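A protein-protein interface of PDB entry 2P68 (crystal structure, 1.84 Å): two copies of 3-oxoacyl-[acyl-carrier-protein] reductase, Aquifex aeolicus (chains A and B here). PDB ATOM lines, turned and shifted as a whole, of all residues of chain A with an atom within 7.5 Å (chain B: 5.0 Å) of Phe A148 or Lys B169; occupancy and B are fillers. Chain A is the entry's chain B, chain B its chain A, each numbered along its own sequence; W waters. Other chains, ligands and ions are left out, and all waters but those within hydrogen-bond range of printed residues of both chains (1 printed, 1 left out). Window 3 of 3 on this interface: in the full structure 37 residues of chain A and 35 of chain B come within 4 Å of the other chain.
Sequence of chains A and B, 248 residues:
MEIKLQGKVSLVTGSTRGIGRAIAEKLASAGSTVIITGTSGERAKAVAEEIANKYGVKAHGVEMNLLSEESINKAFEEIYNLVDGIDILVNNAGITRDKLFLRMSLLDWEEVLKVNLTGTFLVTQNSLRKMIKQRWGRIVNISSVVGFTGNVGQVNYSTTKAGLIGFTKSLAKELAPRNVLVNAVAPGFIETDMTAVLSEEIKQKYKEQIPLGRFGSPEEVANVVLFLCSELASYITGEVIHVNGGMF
Among the printed residues, merely in contact across the chains: Phe A148 with Lys B169 (3.1 Å), Gly A150 with Ser B170 (3.2 Å), Val A155 with Phe B167 (3.4 Å), Ala A162 with Gly B166 (3.6 Å), Val A155 with Ser B170 (3.7 Å), Thr A149 with Lys B169 (3.7 Å), Val A155 with Leu B171 (3.8 Å), Gly A150 with Lys B173 (3.8 Å) and Val A152 with Lys B173 (3.9 Å).
Of the 11 printed residues of chain B, 6 touch a printed residue of chain A.
Hydrophobic or aromatic side chains of chain B that line the printed part of chain A: Phe B167.
Of the 23 printed residues of chain A, 8 touch a printed residue of chain B.
Printed residues of chain A that touch a printed residue of chain B: Phe A148, Thr A149, Gly A150, Asn A151, Val A152, Val A155, Ser A158 and Ala A162.
Among the printed residues, no Asp or Glu carboxylate lies within 4 Å of a Lys or Arg side-chain nitrogen of the other chain.
The backbone carbonyl oxygen of Gly B166 is in hydrogen-bond range of the side-chain hydroxyl of Ser B170, 3.2 Å away.
O of Val A145 is in hydrogen-bond range of OG1 of Thr A149 (3.4 Å).
O of Gly B238 is in hydrogen-bond range of NZ of Lys B169.
OG of Ser A158 lies within hydrogen-bond range of O of Val A146 (2.8 Å).
Water W1 bridges O of Thr A149 (2.7 Å) and NZ of Lys B173 (2.8 Å).
Positions printed for both chains: 165 and 169.
Of the 13 pairs that touch across the chains among the printed residues, none has its exchanged pair printed and touching as well.
Phe A148 touches just one residue of chain B: Lys B169 (3.1 Å).
Of the printed residues of chain A, Lys B169 touches Phe A148 and Thr A149.
Printed residues of chain B within 4 Å of Thr A149: Lys B169 and Lys B173.
Printed residues of chain B within 4 Å of Val A152: Lys B173.
Ala B172 touches none of the printed residues of chain A.
Ser A143 touches none of the printed residues of chain B.
The nearest printed residue of chain B that does not touch Phe A148 is Gly B166 (6.0 Å).
The nearest residue of chain A that does not touch Lys B169 is Gly A150 (4.1 Å).
NZ of Lys B173 sits close to O of Thr A149 (3.4 Å).
The side-chain hydroxyl of Ser B170 sits close to the side-chain hydroxyl of Ser A158, at 3.1 Å.
O of Gly B166 sits at hydrogen-bond distance from OG of Ser A158.
N of Asn A151 lies within hydrogen-bond range of OG of Ser B170, 3.0 Å away.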
ATOM      1  N   SER A 143      25.057  -0.671   0.692  1.00  0.00           N
ATOM      2  CA  SER A 143      23.965   0.307   0.827  1.00  0.00           C
ATOM      3  C   SER A 143      23.186  -0.042   2.103  1.00  0.00           C
ATOM      4  O   SER A 143      23.789  -0.491   3.085  1.00  0.00           O
ATOM      5  CB  SER A 143      23.077   0.279  -0.425  1.00  0.00           C
ATOM      6  OG  SER A 143      22.025   1.262  -0.406  1.00  0.00           O
ATOM      7  N   SER A 144      21.870   0.165   2.091  1.00  0.00           N
ATOM      8  CA  SER A 144      21.003  -0.165   3.225  1.00  0.00           C
ATOM      9  C   SER A 144      19.559  -0.112   2.788  1.00  0.00           C
ATOM     10  O   SER A 144      19.186   0.695   1.933  1.00  0.00           O
ATOM     11  CB  SER A 144      21.223   0.819   4.390  1.00  0.00           C
ATOM     12  OG  SER A 144      20.204   0.711   5.370  1.00  0.00           O
ATOM     13  N   VAL A 145      18.739  -0.966   3.397  1.00  0.00           N
ATOM     14  CA  VAL A 145      17.313  -0.928   3.158  1.00  0.00           C
ATOM     15  C   VAL A 145      16.764   0.512   3.302  1.00  0.00           C
ATOM     16  O   VAL A 145      15.877   0.906   2.564  1.00  0.00           O
ATOM     17  CB  VAL A 145      16.574  -1.923   4.092  1.00  0.00           C
ATOM     18  CG1 VAL A 145      16.655  -1.468   5.565  1.00  0.00           C
ATOM     19  CG2 VAL A 145      15.132  -2.168   3.612  1.00  0.00           C
ATOM     20  N   VAL A 146      17.309   1.304   4.227  1.00  0.00           N
ATOM     21  CA  VAL A 146      16.755   2.663   4.450  1.00  0.00           C
ATOM     22  C   VAL A 146      17.027   3.628   3.292  1.00  0.00           C
ATOM     23  O   VAL A 146      16.379   4.670   3.176  1.00  0.00           O
ATOM     24  CB  VAL A 146      17.187   3.290   5.812  1.00  0.00           C
ATOM     25  CG1 VAL A 146      16.808   2.371   6.975  1.00  0.00           C
ATOM     26  CG2 VAL A 146      18.668   3.587   5.838  1.00  0.00           C
ATOM     27  N   GLY A 147      17.967   3.267   2.427  1.00  0.00           N
ATOM     28  CA  GLY A 147      18.167   3.989   1.180  1.00  0.00           C
ATOM     29  C   GLY A 147      16.962   3.843   0.261  1.00  0.00           C
ATOM     30  O   GLY A 147      16.718   4.702  -0.583  1.00  0.00           O
ATOM     31  N   PHE A 148      16.203   2.763   0.452  1.00  0.00           N
ATOM     32  CA  PHE A 148      15.055   2.451  -0.390  1.00  0.00           C
ATOM     33  C   PHE A 148      13.742   2.873   0.229  1.00  0.00           C
ATOM     34  O   PHE A 148      12.862   3.381  -0.461  1.00  0.00           O
ATOM     35  CB  PHE A 148      15.030   0.958  -0.730  1.00  0.00           C
ATOM     36  CG  PHE A 148      16.132   0.555  -1.649  1.00  0.00           C
ATOM     37  CD1 PHE A 148      15.908   0.456  -3.029  1.00  0.00           C
ATOM     38  CD2 PHE A 148      17.405   0.324  -1.151  1.00  0.00           C
ATOM     39  CE1 PHE A 148      16.945   0.114  -3.884  1.00  0.00           C
ATOM     40  CE2 PHE A 148      18.449  -0.009  -1.998  1.00  0.00           C
ATOM     41  CZ  PHE A 148      18.214  -0.130  -3.368  1.00  0.00           C
ATOM     42  N   THR A 149      13.624   2.664   1.533  1.00  0.00           N
ATOM     43  CA  THR A 149      12.388   2.944   2.255  1.00  0.00           C
ATOM     44  C   THR A 149      12.362   4.354   2.832  1.00  0.00           C
ATOM     45  O   THR A 149      11.284   4.919   3.061  1.00  0.00           O
ATOM     46  CB  THR A 149      12.188   1.940   3.416  1.00  0.00           C
ATOM     47  OG1 THR A 149      13.253   2.073   4.371  1.00  0.00           O
ATOM     48  CG2 THR A 149      12.150   0.504   2.893  1.00  0.00           C
ATOM     49  N   GLY A 150      13.551   4.915   3.058  1.00  0.00           N
ATOM     50  CA  GLY A 150      13.701   6.095   3.905  1.00  0.00           C
ATOM     51  C   GLY A 150      13.597   5.695   5.368  1.00  0.00           C
ATOM     52  O   GLY A 150      13.115   4.601   5.679  1.00  0.00           O
ATOM     53  N   ASN A 151      14.057   6.568   6.265  1.00  0.00           N
ATOM     54  CA  ASN A 151      13.945   6.335   7.707  1.00  0.00           C
ATOM     55  C   ASN A 151      13.981   7.625   8.519  1.00  0.00           C
ATOM     56  O   ASN A 151      14.818   8.498   8.279  1.00  0.00           O
ATOM     57  CB  ASN A 151      15.046   5.391   8.207  1.00  0.00           C
ATOM     58  CG  ASN A 151      14.772   4.872   9.613  1.00  0.00           C
ATOM     59  OD1 ASN A 151      13.613   4.672  10.005  1.00  0.00           O
ATOM     60  ND2 ASN A 151      15.837   4.625  10.369  1.00  0.00           N
ATOM     61  N   VAL A 152      13.066   7.731   9.478  1.00  0.00           N
ATOM     62  CA  VAL A 152      13.007   8.882  10.371  1.00  0.00           C
ATOM     63  C   VAL A 152      14.322   8.997  11.145  1.00  0.00           C
ATOM     64  O   VAL A 152      14.831   8.004  11.668  1.00  0.00           O
ATOM     65  CB  VAL A 152      11.800   8.774  11.335  1.00  0.00           C
ATOM     66  CG1 VAL A 152      11.828   9.891  12.375  1.00  0.00           C
ATOM     67  CG2 VAL A 152      10.492   8.812  10.542  1.00  0.00           C
ATOM     68  N   VAL A 155      17.695  11.245   7.415  1.00  0.00           N
ATOM     69  CA  VAL A 155      17.634  11.862   6.096  1.00  0.00           C
ATOM     70  C   VAL A 155      19.036  11.910   5.453  1.00  0.00           C
ATOM     71  O   VAL A 155      19.179  11.692   4.249  1.00  0.00           O
ATOM     72  CB  VAL A 155      16.987  13.264   6.145  1.00  0.00           C
ATOM     73  CG1 VAL A 155      17.081  13.931   4.793  1.00  0.00           C
ATOM     74  CG2 VAL A 155      15.529  13.163   6.579  1.00  0.00           C
ATOM     75  N   SER A 158      20.195   7.986   4.742  1.00  0.00           N
ATOM     76  CA  SER A 158      19.377   7.464   3.651  1.00  0.00           C
ATOM     77  C   SER A 158      19.717   8.083   2.295  1.00  0.00           C
ATOM     78  O   SER A 158      19.736   7.376   1.283  1.00  0.00           O
ATOM     79  CB  SER A 158      17.890   7.649   3.946  1.00  0.00           C
ATOM     80  OG  SER A 158      17.125   7.293   2.814  1.00  0.00           O
ATOM     81  N   LYS A 161      22.857   6.310   1.160  1.00  0.00           N
ATOM     82  CA  LYS A 161      22.621   4.906   0.790  1.00  0.00           C
ATOM     83  C   LYS A 161      21.801   4.763  -0.497  1.00  0.00           C
ATOM     84  O   LYS A 161      22.024   3.837  -1.287  1.00  0.00           O
ATOM     85  CB  LYS A 161      22.035   4.106   1.975  1.00  0.00           C
ATOM     86  CG  LYS A 161      23.049   3.887   3.143  1.00  0.00           C
ATOM     87  CD  LYS A 161      24.475   3.518   2.643  1.00  0.00           C
ATOM     88  CE  LYS A 161      25.461   3.315   3.792  1.00  0.00           C
ATOM     89  NZ  LYS A 161      26.752   2.666   3.392  1.00  0.00           N
ATOM     90  N   ALA A 162      20.890   5.707  -0.742  1.00  0.00           N
ATOM     91  CA  ALA A 162      20.204   5.790  -2.013  1.00  0.00           C
ATOM     92  C   ALA A 162      21.193   6.239  -3.091  1.00  0.00           C
ATOM     93  O   ALA A 162      21.222   5.683  -4.185  1.00  0.00           O
ATOM     94  CB  ALA A 162      19.038   6.777  -1.943  1.00  0.00           C
ATOM     95  N   ILE A 165      23.243   3.798  -4.912  1.00  0.00           N
ATOM     96  CA  ILE A 165      22.556   3.050  -5.984  1.00  0.00           C
ATOM     97  C   ILE A 165      22.792   3.683  -7.360  1.00  0.00           C
ATOM     98  O   ILE A 165      23.150   2.976  -8.306  1.00  0.00           O
ATOM     99  CB  ILE A 165      21.050   2.811  -5.694  1.00  0.00           C
ATOM    100  CG1 ILE A 165      20.845   2.216  -4.291  1.00  0.00           C
ATOM    101  CG2 ILE A 165      20.423   1.894  -6.769  1.00  0.00           C
ATOM    102  CD1 ILE A 165      21.760   1.050  -3.939  1.00  0.00           C
ATOM    103  N   LYS A 169      24.917   1.915 -10.431  1.00  0.00           N
ATOM    104  CA  LYS A 169      24.367   1.695 -11.778  1.00  0.00           C
ATOM    105  C   LYS A 169      25.169   2.414 -12.841  1.00  0.00           C
ATOM    106  O   LYS A 169      25.417   1.855 -13.919  1.00  0.00           O
ATOM    107  CB  LYS A 169      22.892   2.080 -11.833  1.00  0.00           C
ATOM    108  CG  LYS A 169      22.036   1.123 -11.000  1.00  0.00           C
ATOM    109  CD  LYS A 169      20.566   1.280 -11.306  1.00  0.00           C
ATOM    110  CE  LYS A 169      19.745   0.272 -10.517  1.00  0.00           C
ATOM    111  NZ  LYS A 169      19.903  -1.130 -11.032  1.00  0.00           N
ATOM    112  N   ALA A 184      25.628  -3.648  -5.635  1.00  0.00           N
ATOM    113  CA  ALA A 184      25.401  -3.185  -4.274  1.00  0.00           C
ATOM    114  C   ALA A 184      24.732  -4.294  -3.493  1.00  0.00           C
ATOM    115  O   ALA A 184      23.998  -5.114  -4.057  1.00  0.00           O
ATOM    116  CB  ALA A 184      24.513  -1.942  -4.263  1.00  0.00           C
ATOM    117  N   VAL A 185      24.991  -4.309  -2.191  1.00  0.00           N
ATOM    118  CA  VAL A 185      24.267  -5.162  -1.268  1.00  0.00           C
ATOM    119  C   VAL A 185      23.550  -4.204  -0.330  1.00  0.00           C
ATOM    120  O   VAL A 185      24.159  -3.246   0.154  1.00  0.00           O
ATOM    121  CB  VAL A 185      25.217  -6.088  -0.480  1.00  0.00           C
ATOM    122  CG1 VAL A 185      24.477  -6.805   0.671  1.00  0.00           C
ATOM    123  CG2 VAL A 185      25.884  -7.091  -1.424  1.00  0.00           C
ATOM    124  N   ALA A 186      22.255  -4.438  -0.104  1.00  0.00           N
ATOM    125  CA  ALA A 186      21.468  -3.598   0.785  1.00  0.00           C
ATOM    126  C   ALA A 186      20.962  -4.413   1.977  1.00  0.00           C
ATOM    127  O   ALA A 186      19.892  -5.033   1.907  1.00  0.00           O
ATOM    128  CB  ALA A 186      20.308  -2.933   0.028  1.00  0.00           C
ATOM    129  N   PRO A 187      21.744  -4.445   3.072  1.00  0.00           N
ATOM    130  CA  PRO A 187      21.331  -5.161   4.291  1.00  0.00           C
ATOM    131  C   PRO A 187      20.105  -4.521   4.928  1.00  0.00           C
ATOM    132  O   PRO A 187      19.918  -3.297   4.836  1.00  0.00           O
ATOM    133  CB  PRO A 187      22.535  -5.001   5.228  1.00  0.00           C
ATOM    134  CG  PRO A 187      23.671  -4.578   4.357  1.00  0.00           C
ATOM    135  CD  PRO A 187      23.055  -3.796   3.238  1.00  0.00           C
ATOM    136  N   VAL A 240      21.327  -4.411  -7.315  1.00  0.00           N
ATOM    137  CA  VAL A 240      21.302  -4.342  -5.860  1.00  0.00           C
ATOM    138  C   VAL A 240      20.732  -5.654  -5.363  1.00  0.00           C
ATOM    139  O   VAL A 240      19.662  -6.101  -5.828  1.00  0.00           O
ATOM    140  CB  VAL A 240      20.382  -3.201  -5.361  1.00  0.00           C
ATOM    141  CG1 VAL A 240      20.432  -3.100  -3.822  1.00  0.00           C
ATOM    142  CG2 VAL A 240      20.787  -1.878  -5.973  1.00  0.00           C
ATOM    143  N   ILE A 241      21.439  -6.298  -4.439  1.00  0.00           N
ATOM    144  CA  ILE A 241      20.868  -7.466  -3.780  1.00  0.00           C
ATOM    145  C   ILE A 241      20.430  -7.083  -2.367  1.00  0.00           C
ATOM    146  O   ILE A 241      21.235  -6.641  -1.552  1.00  0.00           O
ATOM    147  CB  ILE A 241      21.824  -8.681  -3.763  1.00  0.00           C
ATOM    148  CG1 ILE A 241      22.237  -9.070  -5.207  1.00  0.00           C
ATOM    149  CG2 ILE A 241      21.164  -9.831  -2.999  1.00  0.00           C
ATOM    150  CD1 ILE A 241      23.046 -10.356  -5.308  1.00  0.00           C
ATOM    151  N   HIS A 242      19.138  -7.225  -2.107  1.00  0.00           N
ATOM    152  CA  HIS A 242      18.575  -6.915  -0.804  1.00  0.00           C
ATOM    153  C   HIS A 242      18.714  -8.134   0.109  1.00  0.00           C
ATOM    154  O   HIS A 242      18.368  -9.242  -0.316  1.00  0.00           O
ATOM    155  CB  HIS A 242      17.121  -6.503  -0.972  1.00  0.00           C
ATOM    156  CG  HIS A 242      16.964  -5.168  -1.635  1.00  0.00           C
ATOM    157  ND1 HIS A 242      16.926  -3.926  -1.110  1.00  0.00           N
ATOM    158  CD2 HIS A 242      16.861  -5.010  -3.002  1.00  0.00           C
ATOM    159  CE1 HIS A 242      16.792  -3.045  -2.154  1.00  0.00           C
ATOM    160  NE2 HIS A 242      16.759  -3.720  -3.286  1.00  0.00           N
ATOM    161  N   ILE B 165      16.243  10.683  -3.939  1.00  0.00           N
ATOM    162  CA  ILE B 165      15.111   9.784  -3.670  1.00  0.00           C
ATOM    163  C   ILE B 165      15.092   9.344  -2.196  1.00  0.00           C
ATOM    164  O   ILE B 165      14.030   9.331  -1.564  1.00  0.00           O
ATOM    165  CB  ILE B 165      15.073   8.572  -4.631  1.00  0.00           C
ATOM    166  CG1 ILE B 165      15.248   9.015  -6.094  1.00  0.00           C
ATOM    167  CG2 ILE B 165      13.780   7.769  -4.440  1.00  0.00           C
ATOM    168  CD1 ILE B 165      14.280  10.132  -6.573  1.00  0.00           C
ATOM    169  N   GLY B 166      16.259   8.981  -1.656  1.00  0.00           N
ATOM    170  CA  GLY B 166      16.393   8.677  -0.231  1.00  0.00           C
ATOM    171  C   GLY B 166      16.035   9.896   0.601  1.00  0.00           C
ATOM    172  O   GLY B 166      15.333   9.785   1.607  1.00  0.00           O
ATOM    173  N   PHE B 167      16.551  11.055   0.190  1.00  0.00           N
ATOM    174  CA  PHE B 167      16.206  12.337   0.819  1.00  0.00           C
ATOM    175  C   PHE B 167      14.686  12.509   0.867  1.00  0.00           C
ATOM    176  O   PHE B 167      14.119  12.771   1.925  1.00  0.00           O
ATOM    177  CB  PHE B 167      16.857  13.483   0.039  1.00  0.00           C
ATOM    178  CG  PHE B 167      16.608  14.849   0.623  1.00  0.00           C
ATOM    179  CD1 PHE B 167      17.401  15.332   1.666  1.00  0.00           C
ATOM    180  CD2 PHE B 167      15.609  15.668   0.102  1.00  0.00           C
ATOM    181  CE1 PHE B 167      17.184  16.604   2.186  1.00  0.00           C
ATOM    182  CE2 PHE B 167      15.376  16.937   0.619  1.00  0.00           C
ATOM    183  CZ  PHE B 167      16.169  17.412   1.660  1.00  0.00           C
ATOM    184  N   THR B 168      14.038  12.325  -0.280  1.00  0.00           N
ATOM    185  CA  THR B 168      12.586  12.508  -0.408  1.00  0.00           C
ATOM    186  C   THR B 168      11.810  11.550   0.501  1.00  0.00           C
ATOM    187  O   THR B 168      10.946  11.982   1.257  1.00  0.00           O
ATOM    188  CB  THR B 168      12.134  12.335  -1.885  1.00  0.00           C
ATOM    189  OG1 THR B 168      12.763  13.339  -2.690  1.00  0.00           O
ATOM    190  CG2 THR B 168      10.624  12.465  -2.029  1.00  0.00           C
ATOM    191  N   LYS B 169      12.128  10.256   0.441  1.00  0.00           N
ATOM    192  CA  LYS B 169      11.378   9.271   1.232  1.00  0.00           C
ATOM    193  C   LYS B 169      11.561   9.434   2.743  1.00  0.00           C
ATOM    194  O   LYS B 169      10.601   9.267   3.500  1.00  0.00           O
ATOM    195  CB  LYS B 169      11.709   7.849   0.796  1.00  0.00           C
ATOM    196  CG  LYS B 169      11.192   7.527  -0.602  1.00  0.00           C
ATOM    197  CD  LYS B 169      11.227   6.036  -0.874  1.00  0.00           C
ATOM    198  CE  LYS B 169      10.714   5.685  -2.267  1.00  0.00           C
ATOM    199  NZ  LYS B 169       9.282   6.059  -2.495  1.00  0.00           N
ATOM    200  N   SER B 170      12.777   9.765   3.174  1.00  0.00           N
ATOM    201  CA  SER B 170      13.058  10.001   4.595  1.00  0.00           C
ATOM    202  C   SER B 170      12.381  11.262   5.125  1.00  0.00           C
ATOM    203  O   SER B 170      11.735  11.248   6.182  1.00  0.00           O
ATOM    204  CB  SER B 170      14.557  10.088   4.833  1.00  0.00           C
ATOM    205  OG  SER B 170      15.141   8.809   4.674  1.00  0.00           O
ATOM    206  N   LEU B 171      12.535  12.358   4.396  1.00  0.00           N
ATOM    207  CA  LEU B 171      11.919  13.609   4.819  1.00  0.00           C
ATOM    208  C   LEU B 171      10.403  13.501   4.812  1.00  0.00           C
ATOM    209  O   LEU B 171       9.735  14.064   5.673  1.00  0.00           O
ATOM    210  CB  LEU B 171      12.382  14.766   3.944  1.00  0.00           C
ATOM    211  CG  LEU B 171      12.002  16.162   4.458  1.00  0.00           C
ATOM    212  CD1 LEU B 171      12.517  16.411   5.886  1.00  0.00           C
ATOM    213  CD2 LEU B 171      12.541  17.198   3.485  1.00  0.00           C
ATOM    214  N   ALA B 172       9.855  12.771   3.845  1.00  0.00           N
ATOM    215  CA  ALA B 172       8.409  12.592   3.783  1.00  0.00           C
ATOM    216  C   ALA B 172       7.889  11.937   5.061  1.00  0.00           C
ATOM    217  O   ALA B 172       6.869  12.349   5.595  1.00  0.00           O
ATOM    218  CB  ALA B 172       8.017  11.760   2.561  1.00  0.00           C
ATOM    219  N   LYS B 173       8.592  10.905   5.531  1.00  0.00           N
ATOM    220  CA  LYS B 173       8.186  10.198   6.736  1.00  0.00           C
ATOM    221  C   LYS B 173       8.249  11.111   7.956  1.00  0.00           C
ATOM    222  O   LYS B 173       7.353  11.089   8.798  1.00  0.00           O
ATOM    223  CB  LYS B 173       9.044   8.945   6.951  1.00  0.00           C
ATOM    224  CG  LYS B 173       8.723   7.802   5.968  1.00  0.00           C
ATOM    225  CD  LYS B 173       9.471   6.527   6.382  1.00  0.00           C
ATOM    226  CE  LYS B 173       9.391   5.428   5.342  1.00  0.00           C
ATOM    227  NZ  LYS B 173       8.220   5.501   4.421  1.00  0.00           N
ATOM    228  N   GLY B 238       6.298  10.941  -0.321  1.00  0.00           N
ATOM    229  CA  GLY B 238       7.381   9.958  -0.387  1.00  0.00           C
ATOM    230  C   GLY B 238       7.490   9.335  -1.767  1.00  0.00           C
ATOM    231  O   GLY B 238       8.160   8.310  -1.931  1.00  0.00           O
ATOM    232  N   GLU B 239       6.827   9.949  -2.748  1.00  0.00           N
ATOM    233  CA  GLU B 239       6.686   9.365  -4.088  1.00  0.00           C
ATOM    234  C   GLU B 239       7.562  10.081  -5.120  1.00  0.00           C
ATOM    235  O   GLU B 239       7.871  11.265  -4.980  1.00  0.00           O
ATOM    236  CB  GLU B 239       5.200   9.360  -4.503  1.00  0.00           C
ATOM    237  CG  GLU B 239       4.881   9.056  -5.997  1.00  0.00           C
ATOM    238  CD  GLU B 239       5.255   7.647  -6.478  1.00  0.00           C
ATOM    239  OE1 GLU B 239       6.230   7.032  -5.975  1.00  0.00           O
ATOM    240  OE2 GLU B 239       4.591   7.180  -7.430  1.00  0.00           O
HETATM  241  O   HOH W   1       8.900   4.025   2.100  1.00  0.00           O
